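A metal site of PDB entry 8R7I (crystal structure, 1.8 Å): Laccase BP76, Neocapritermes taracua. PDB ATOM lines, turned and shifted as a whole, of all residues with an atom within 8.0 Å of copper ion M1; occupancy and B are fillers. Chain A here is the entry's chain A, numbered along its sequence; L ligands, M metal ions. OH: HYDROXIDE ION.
O of Phe 589 sits at hydrogen-bond distance from N of His 526.
O of His 591 sits at hydrogen-bond distance from N of His 524 (2.9 Å).
A ring nitrogen (ND1) of His 526 sits at hydrogen-bond distance from the side-chain carboxylate (OD2) of Asp 129.
Of the 20 residues printed, 3 come within 4 Å of copper ion M1.
Copper ion M1 is bound by a ring nitrogen (NE2) of His 591 (2.0 Å), a ring nitrogen (NE2) of His 526 (2.1 Å), a ring nitrogen (NE2) of His 162 (2.1 Å) and an oxygen (O) of the ligand (2.3 Å).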
ATOM      1  N   HIS A 116      -3.012  17.761  -1.239  1.00  0.00           N
ATOM      2  CA  HIS A 116      -1.665  17.606  -0.668  1.00  0.00           C
ATOM      3  C   HIS A 116      -1.227  16.129  -0.806  1.00  0.00           C
ATOM      4  O   HIS A 116      -2.040  15.186  -0.583  1.00  0.00           O
ATOM      5  CB  HIS A 116      -1.674  18.070   0.797  1.00  0.00           C
ATOM      6  CG  HIS A 116      -0.442  17.681   1.516  1.00  0.00           C
ATOM      7  ND1 HIS A 116       0.811  18.134   1.119  1.00  0.00           N
ATOM      8  CD2 HIS A 116      -0.251  16.922   2.629  1.00  0.00           C
ATOM      9  CE1 HIS A 116       1.717  17.657   1.963  1.00  0.00           C
ATOM     10  NE2 HIS A 116       1.096  16.950   2.859  1.00  0.00           N
ATOM     11  N   HIS A 118       0.724  13.801   0.844  1.00  0.00           N
ATOM     12  CA  HIS A 118       1.226  13.626   2.212  1.00  0.00           C
ATOM     13  C   HIS A 118       2.351  12.570   2.226  1.00  0.00           C
ATOM     14  O   HIS A 118       2.130  11.395   1.906  1.00  0.00           O
ATOM     15  CB  HIS A 118       0.039  13.272   3.114  1.00  0.00           C
ATOM     16  CG  HIS A 118       0.399  13.007   4.542  1.00  0.00           C
ATOM     17  ND1 HIS A 118      -0.346  13.540   5.555  1.00  0.00           N
ATOM     18  CD2 HIS A 118       1.297  12.199   5.137  1.00  0.00           C
ATOM     19  CE1 HIS A 118       0.155  13.113   6.752  1.00  0.00           C
ATOM     20  NE2 HIS A 118       1.146  12.311   6.519  1.00  0.00           N
ATOM     21  N   ASP A 129       3.053  21.210  -3.371  1.00  0.00           N
ATOM     22  CA  ASP A 129       2.759  20.607  -2.067  1.00  0.00           C
ATOM     23  C   ASP A 129       1.255  20.580  -1.754  1.00  0.00           C
ATOM     24  O   ASP A 129       0.816  19.714  -0.968  1.00  0.00           O
ATOM     25  CB  ASP A 129       3.553  21.253  -0.926  1.00  0.00           C
ATOM     26  CG  ASP A 129       3.583  20.397   0.353  1.00  0.00           C
ATOM     27  OD1 ASP A 129       3.782  19.146   0.221  1.00  0.00           O
ATOM     28  OD2 ASP A 129       3.414  20.957   1.437  1.00  0.00           O
ATOM     29  N   GLY A 130       0.467  21.518  -2.318  1.00  0.00           N
ATOM     30  CA  GLY A 130      -0.997  21.468  -2.213  1.00  0.00           C
ATOM     31  C   GLY A 130      -1.588  22.151  -0.980  1.00  0.00           C
ATOM     32  O   GLY A 130      -2.683  21.765  -0.565  1.00  0.00           O
ATOM     33  N   VAL A 131      -0.890  23.149  -0.385  1.00  0.00           N
ATOM     34  CA  VAL A 131      -1.388  23.855   0.798  1.00  0.00           C
ATOM     35  C   VAL A 131      -1.878  25.261   0.405  1.00  0.00           C
ATOM     36  O   VAL A 131      -1.071  26.136   0.030  1.00  0.00           O
ATOM     37  CB  VAL A 131      -0.362  23.980   1.935  1.00  0.00           C
ATOM     38  CG1 VAL A 131      -0.982  24.678   3.143  1.00  0.00           C
ATOM     39  CG2 VAL A 131       0.216  22.620   2.311  1.00  0.00           C
ATOM     40  N   LEU A 134      -0.105  28.776   1.214  1.00  0.00           N
ATOM     41  CA  LEU A 134       1.273  28.490   1.637  1.00  0.00           C
ATOM     42  C   LEU A 134       2.134  28.184   0.414  1.00  0.00           C
ATOM     43  O   LEU A 134       3.076  28.922   0.169  1.00  0.00           O
ATOM     44  CB  LEU A 134       1.294  27.355   2.693  1.00  0.00           C
ATOM     45  CG  LEU A 134       2.607  27.256   3.455  1.00  0.00           C
ATOM     46  CD1 LEU A 134       2.877  28.560   4.264  1.00  0.00           C
ATOM     47  CD2 LEU A 134       2.594  26.061   4.399  1.00  0.00           C
ATOM     48  N   HIS A 160      -4.767  13.812   0.078  1.00  0.00           N
ATOM     49  CA  HIS A 160      -6.082  14.280   0.537  1.00  0.00           C
ATOM     50  C   HIS A 160      -6.252  15.740   0.211  1.00  0.00           C
ATOM     51  O   HIS A 160      -5.255  16.469   0.073  1.00  0.00           O
ATOM     52  CB  HIS A 160      -6.274  13.993   2.046  1.00  0.00           C
ATOM     53  CG  HIS A 160      -5.196  14.596   2.889  1.00  0.00           C
ATOM     54  ND1 HIS A 160      -5.269  15.871   3.368  1.00  0.00           N
ATOM     55  CD2 HIS A 160      -4.047  14.080   3.377  1.00  0.00           C
ATOM     56  CE1 HIS A 160      -4.176  16.133   4.129  1.00  0.00           C
ATOM     57  NE2 HIS A 160      -3.458  15.015   4.171  1.00  0.00           N
ATOM     58  N   SER A 161      -7.511  16.201   0.184  1.00  0.00           N
ATOM     59  CA  SER A 161      -7.787  17.624   0.141  1.00  0.00           C
ATOM     60  C   SER A 161      -7.120  18.269   1.355  1.00  0.00           C
ATOM     61  O   SER A 161      -7.241  17.726   2.480  1.00  0.00           O
ATOM     62  CB  SER A 161      -9.253  17.941   0.135  1.00  0.00           C
ATOM     63  OG  SER A 161      -9.404  19.327   0.316  1.00  0.00           O
ATOM     64  N   HIS A 162      -6.427  19.380   1.127  1.00  0.00           N
ATOM     65  CA  HIS A 162      -5.866  20.218   2.202  1.00  0.00           C
ATOM     66  C   HIS A 162      -6.661  21.527   2.299  1.00  0.00           C
ATOM     67  O   HIS A 162      -6.118  22.548   2.781  1.00  0.00           O
ATOM     68  CB  HIS A 162      -4.357  20.427   1.935  1.00  0.00           C
ATOM     69  CG  HIS A 162      -3.569  20.500   3.210  1.00  0.00           C
ATOM     70  ND1 HIS A 162      -3.740  21.562   4.098  1.00  0.00           N
ATOM     71  CD2 HIS A 162      -2.665  19.656   3.778  1.00  0.00           C
ATOM     72  CE1 HIS A 162      -2.918  21.364   5.134  1.00  0.00           C
ATOM     73  NE2 HIS A 162      -2.259  20.220   4.932  1.00  0.00           N
ATOM     74  N   HIS A 524       2.304  16.453  12.215  1.00  0.00           N
ATOM     75  CA  HIS A 524       2.778  16.084  10.898  1.00  0.00           C
ATOM     76  C   HIS A 524       3.557  17.261  10.335  1.00  0.00           C
ATOM     77  O   HIS A 524       3.067  18.383  10.385  1.00  0.00           O
ATOM     78  CB  HIS A 524       1.588  15.679  10.009  1.00  0.00           C
ATOM     79  CG  HIS A 524       1.961  15.633   8.573  1.00  0.00           C
ATOM     80  ND1 HIS A 524       2.922  14.763   8.097  1.00  0.00           N
ATOM     81  CD2 HIS A 524       1.465  16.281   7.499  1.00  0.00           C
ATOM     82  CE1 HIS A 524       3.030  14.928   6.791  1.00  0.00           C
ATOM     83  NE2 HIS A 524       2.136  15.822   6.450  1.00  0.00           N
ATOM     84  N   LEU A 525       4.756  16.979   9.824  1.00  0.00           N
ATOM     85  CA  LEU A 525       5.609  17.968   9.147  1.00  0.00           C
ATOM     86  C   LEU A 525       5.606  17.673   7.657  1.00  0.00           C
ATOM     87  O   LEU A 525       6.050  16.601   7.254  1.00  0.00           O
ATOM     88  CB  LEU A 525       7.044  17.822   9.706  1.00  0.00           C
ATOM     89  CG  LEU A 525       8.079  18.765   9.068  1.00  0.00           C
ATOM     90  CD1 LEU A 525       7.693  20.222   9.261  1.00  0.00           C
ATOM     91  CD2 LEU A 525       9.452  18.461   9.667  1.00  0.00           C
ATOM     92  N   HIS A 526       5.245  18.675   6.851  1.00  0.00           N
ATOM     93  CA  HIS A 526       5.387  18.651   5.393  1.00  0.00           C
ATOM     94  C   HIS A 526       6.860  18.735   4.982  1.00  0.00           C
ATOM     95  O   HIS A 526       7.666  19.329   5.704  1.00  0.00           O
ATOM     96  CB  HIS A 526       4.626  19.791   4.729  1.00  0.00           C
ATOM     97  CG  HIS A 526       3.128  19.739   4.809  1.00  0.00           C
ATOM     98  ND1 HIS A 526       2.339  20.129   3.717  1.00  0.00           N
ATOM     99  CD2 HIS A 526       2.274  19.426   5.810  1.00  0.00           C
ATOM    100  CE1 HIS A 526       1.053  19.962   4.058  1.00  0.00           C
ATOM    101  NE2 HIS A 526       1.029  19.561   5.357  1.00  0.00           N
ATOM    102  N   TRP A 588       6.988  25.070   5.003  1.00  0.00           N
ATOM    103  CA  TRP A 588       6.568  23.730   5.386  1.00  0.00           C
ATOM    104  C   TRP A 588       5.636  23.782   6.587  1.00  0.00           C
ATOM    105  O   TRP A 588       6.032  24.241   7.663  1.00  0.00           O
ATOM    106  CB  TRP A 588       7.784  22.850   5.646  1.00  0.00           C
ATOM    107  CG  TRP A 588       8.683  22.767   4.441  1.00  0.00           C
ATOM    108  CD1 TRP A 588       9.929  23.305   4.317  1.00  0.00           C
ATOM    109  CD2 TRP A 588       8.380  22.179   3.170  1.00  0.00           C
ATOM    110  NE1 TRP A 588      10.439  23.054   3.083  1.00  0.00           N
ATOM    111  CE2 TRP A 588       9.509  22.381   2.337  1.00  0.00           C
ATOM    112  CE3 TRP A 588       7.253  21.518   2.632  1.00  0.00           C
ATOM    113  CZ2 TRP A 588       9.588  21.913   1.035  1.00  0.00           C
ATOM    114  CZ3 TRP A 588       7.330  21.063   1.324  1.00  0.00           C
ATOM    115  CH2 TRP A 588       8.489  21.229   0.553  1.00  0.00           C
ATOM    116  N   PHE A 589       4.407  23.311   6.388  1.00  0.00           N
ATOM    117  CA  PHE A 589       3.401  23.232   7.429  1.00  0.00           C
ATOM    118  C   PHE A 589       3.791  22.153   8.440  1.00  0.00           C
ATOM    119  O   PHE A 589       4.245  21.063   8.078  1.00  0.00           O
ATOM    120  CB  PHE A 589       2.025  22.916   6.801  1.00  0.00           C
ATOM    121  CG  PHE A 589       0.858  23.792   7.198  1.00  0.00           C
ATOM    122  CD1 PHE A 589       0.926  24.763   8.193  1.00  0.00           C
ATOM    123  CD2 PHE A 589      -0.376  23.551   6.609  1.00  0.00           C
ATOM    124  CE1 PHE A 589      -0.169  25.532   8.527  1.00  0.00           C
ATOM    125  CE2 PHE A 589      -1.473  24.357   6.938  1.00  0.00           C
ATOM    126  CZ  PHE A 589      -1.377  25.337   7.876  1.00  0.00           C
ATOM    127  N   LEU A 590       3.599  22.470   9.734  1.00  0.00           N
ATOM    128  CA  LEU A 590       3.712  21.562  10.863  1.00  0.00           C
ATOM    129  C   LEU A 590       2.449  21.689  11.696  1.00  0.00           C
ATOM    130  O   LEU A 590       2.179  22.787  12.207  1.00  0.00           O
ATOM    131  CB  LEU A 590       4.924  21.906  11.717  1.00  0.00           C
ATOM    132  CG  LEU A 590       5.029  21.131  13.039  1.00  0.00           C
ATOM    133  CD1 LEU A 590       5.065  19.670  12.794  1.00  0.00           C
ATOM    134  CD2 LEU A 590       6.302  21.569  13.820  1.00  0.00           C
ATOM    135  N   HIS A 591       1.621  20.637  11.767  1.00  0.00           N
ATOM    136  CA  HIS A 591       0.283  20.823  12.359  1.00  0.00           C
ATOM    137  C   HIS A 591      -0.273  19.512  12.896  1.00  0.00           C
ATOM    138  O   HIS A 591       0.172  18.403  12.498  1.00  0.00           O
ATOM    139  CB  HIS A 591      -0.652  21.454  11.336  1.00  0.00           C
ATOM    140  CG  HIS A 591      -0.918  20.579  10.181  1.00  0.00           C
ATOM    141  ND1 HIS A 591      -1.880  19.570  10.238  1.00  0.00           N
ATOM    142  CD2 HIS A 591      -0.378  20.532   8.930  1.00  0.00           C
ATOM    143  CE1 HIS A 591      -1.904  18.947   9.045  1.00  0.00           C
ATOM    144  NE2 HIS A 591      -1.035  19.547   8.251  1.00  0.00           N
ATOM    145  N   CYS A 592      -1.261  19.653  13.796  1.00  0.00           N
ATOM    146  CA  CYS A 592      -1.995  18.495  14.266  1.00  0.00           C
ATOM    147  C   CYS A 592      -2.773  17.948  13.063  1.00  0.00           C
ATOM    148  O   CYS A 592      -3.379  18.736  12.359  1.00  0.00           O
ATOM    149  CB  CYS A 592      -2.910  18.826  15.413  1.00  0.00           C
ATOM    150  SG  CYS A 592      -3.804  17.358  15.908  1.00  0.00           S
ATOM    151  N   HIS A 593      -2.702  16.629  12.818  1.00  0.00           N
ATOM    152  CA  HIS A 593      -3.357  16.039  11.648  1.00  0.00           C
ATOM    153  C   HIS A 593      -4.858  15.826  11.904  1.00  0.00           C
ATOM    154  O   HIS A 593      -5.617  15.611  10.930  1.00  0.00           O
ATOM    155  CB  HIS A 593      -2.641  14.733  11.210  1.00  0.00           C
ATOM    156  CG  HIS A 593      -2.828  14.519   9.721  1.00  0.00           C
ATOM    157  ND1 HIS A 593      -3.909  13.815   9.223  1.00  0.00           N
ATOM    158  CD2 HIS A 593      -2.113  14.945   8.659  1.00  0.00           C
ATOM    159  CE1 HIS A 593      -3.845  13.810   7.912  1.00  0.00           C
ATOM    160  NE2 HIS A 593      -2.732  14.452   7.525  1.00  0.00           N
ATOM    161  N   LEU A 598      -6.486  21.268  13.041  1.00  0.00           N
ATOM    162  CA  LEU A 598      -5.910  22.093  11.978  1.00  0.00           C
ATOM    163  C   LEU A 598      -6.877  23.238  11.655  1.00  0.00           C
ATOM    164  O   LEU A 598      -6.456  24.391  11.506  1.00  0.00           O
ATOM    165  CB  LEU A 598      -5.615  21.242  10.746  1.00  0.00           C
ATOM    166  CG  LEU A 598      -5.226  22.007   9.496  1.00  0.00           C
ATOM    167  CD1 LEU A 598      -3.920  22.740   9.700  1.00  0.00           C
ATOM    168  CD2 LEU A 598      -5.127  21.065   8.292  1.00  0.00           C
ATOM    169  N   ALA A 603      -1.382  24.722  14.341  1.00  0.00           N
ATOM    170  CA  ALA A 603      -0.413  24.681  13.263  1.00  0.00           C
ATOM    171  C   ALA A 603       0.634  25.798  13.428  1.00  0.00           C
ATOM    172  O   ALA A 603       0.302  26.839  14.006  1.00  0.00           O
ATOM    173  CB  ALA A 603      -1.137  24.851  11.944  1.00  0.00           C
HETATM  174  O    OH L   1      -1.558  17.152   5.974  1.00  0.00           O
HETATM  175 CU    CU M   1      -0.845  19.331   6.224  1.00  0.00          CU
HETATM  176 CU    CU M   2       1.706  16.328   4.628  1.00  0.00          CU
HETATM  177 CU    CU M   3      -1.972  14.702   5.539  1.00  0.00          CU
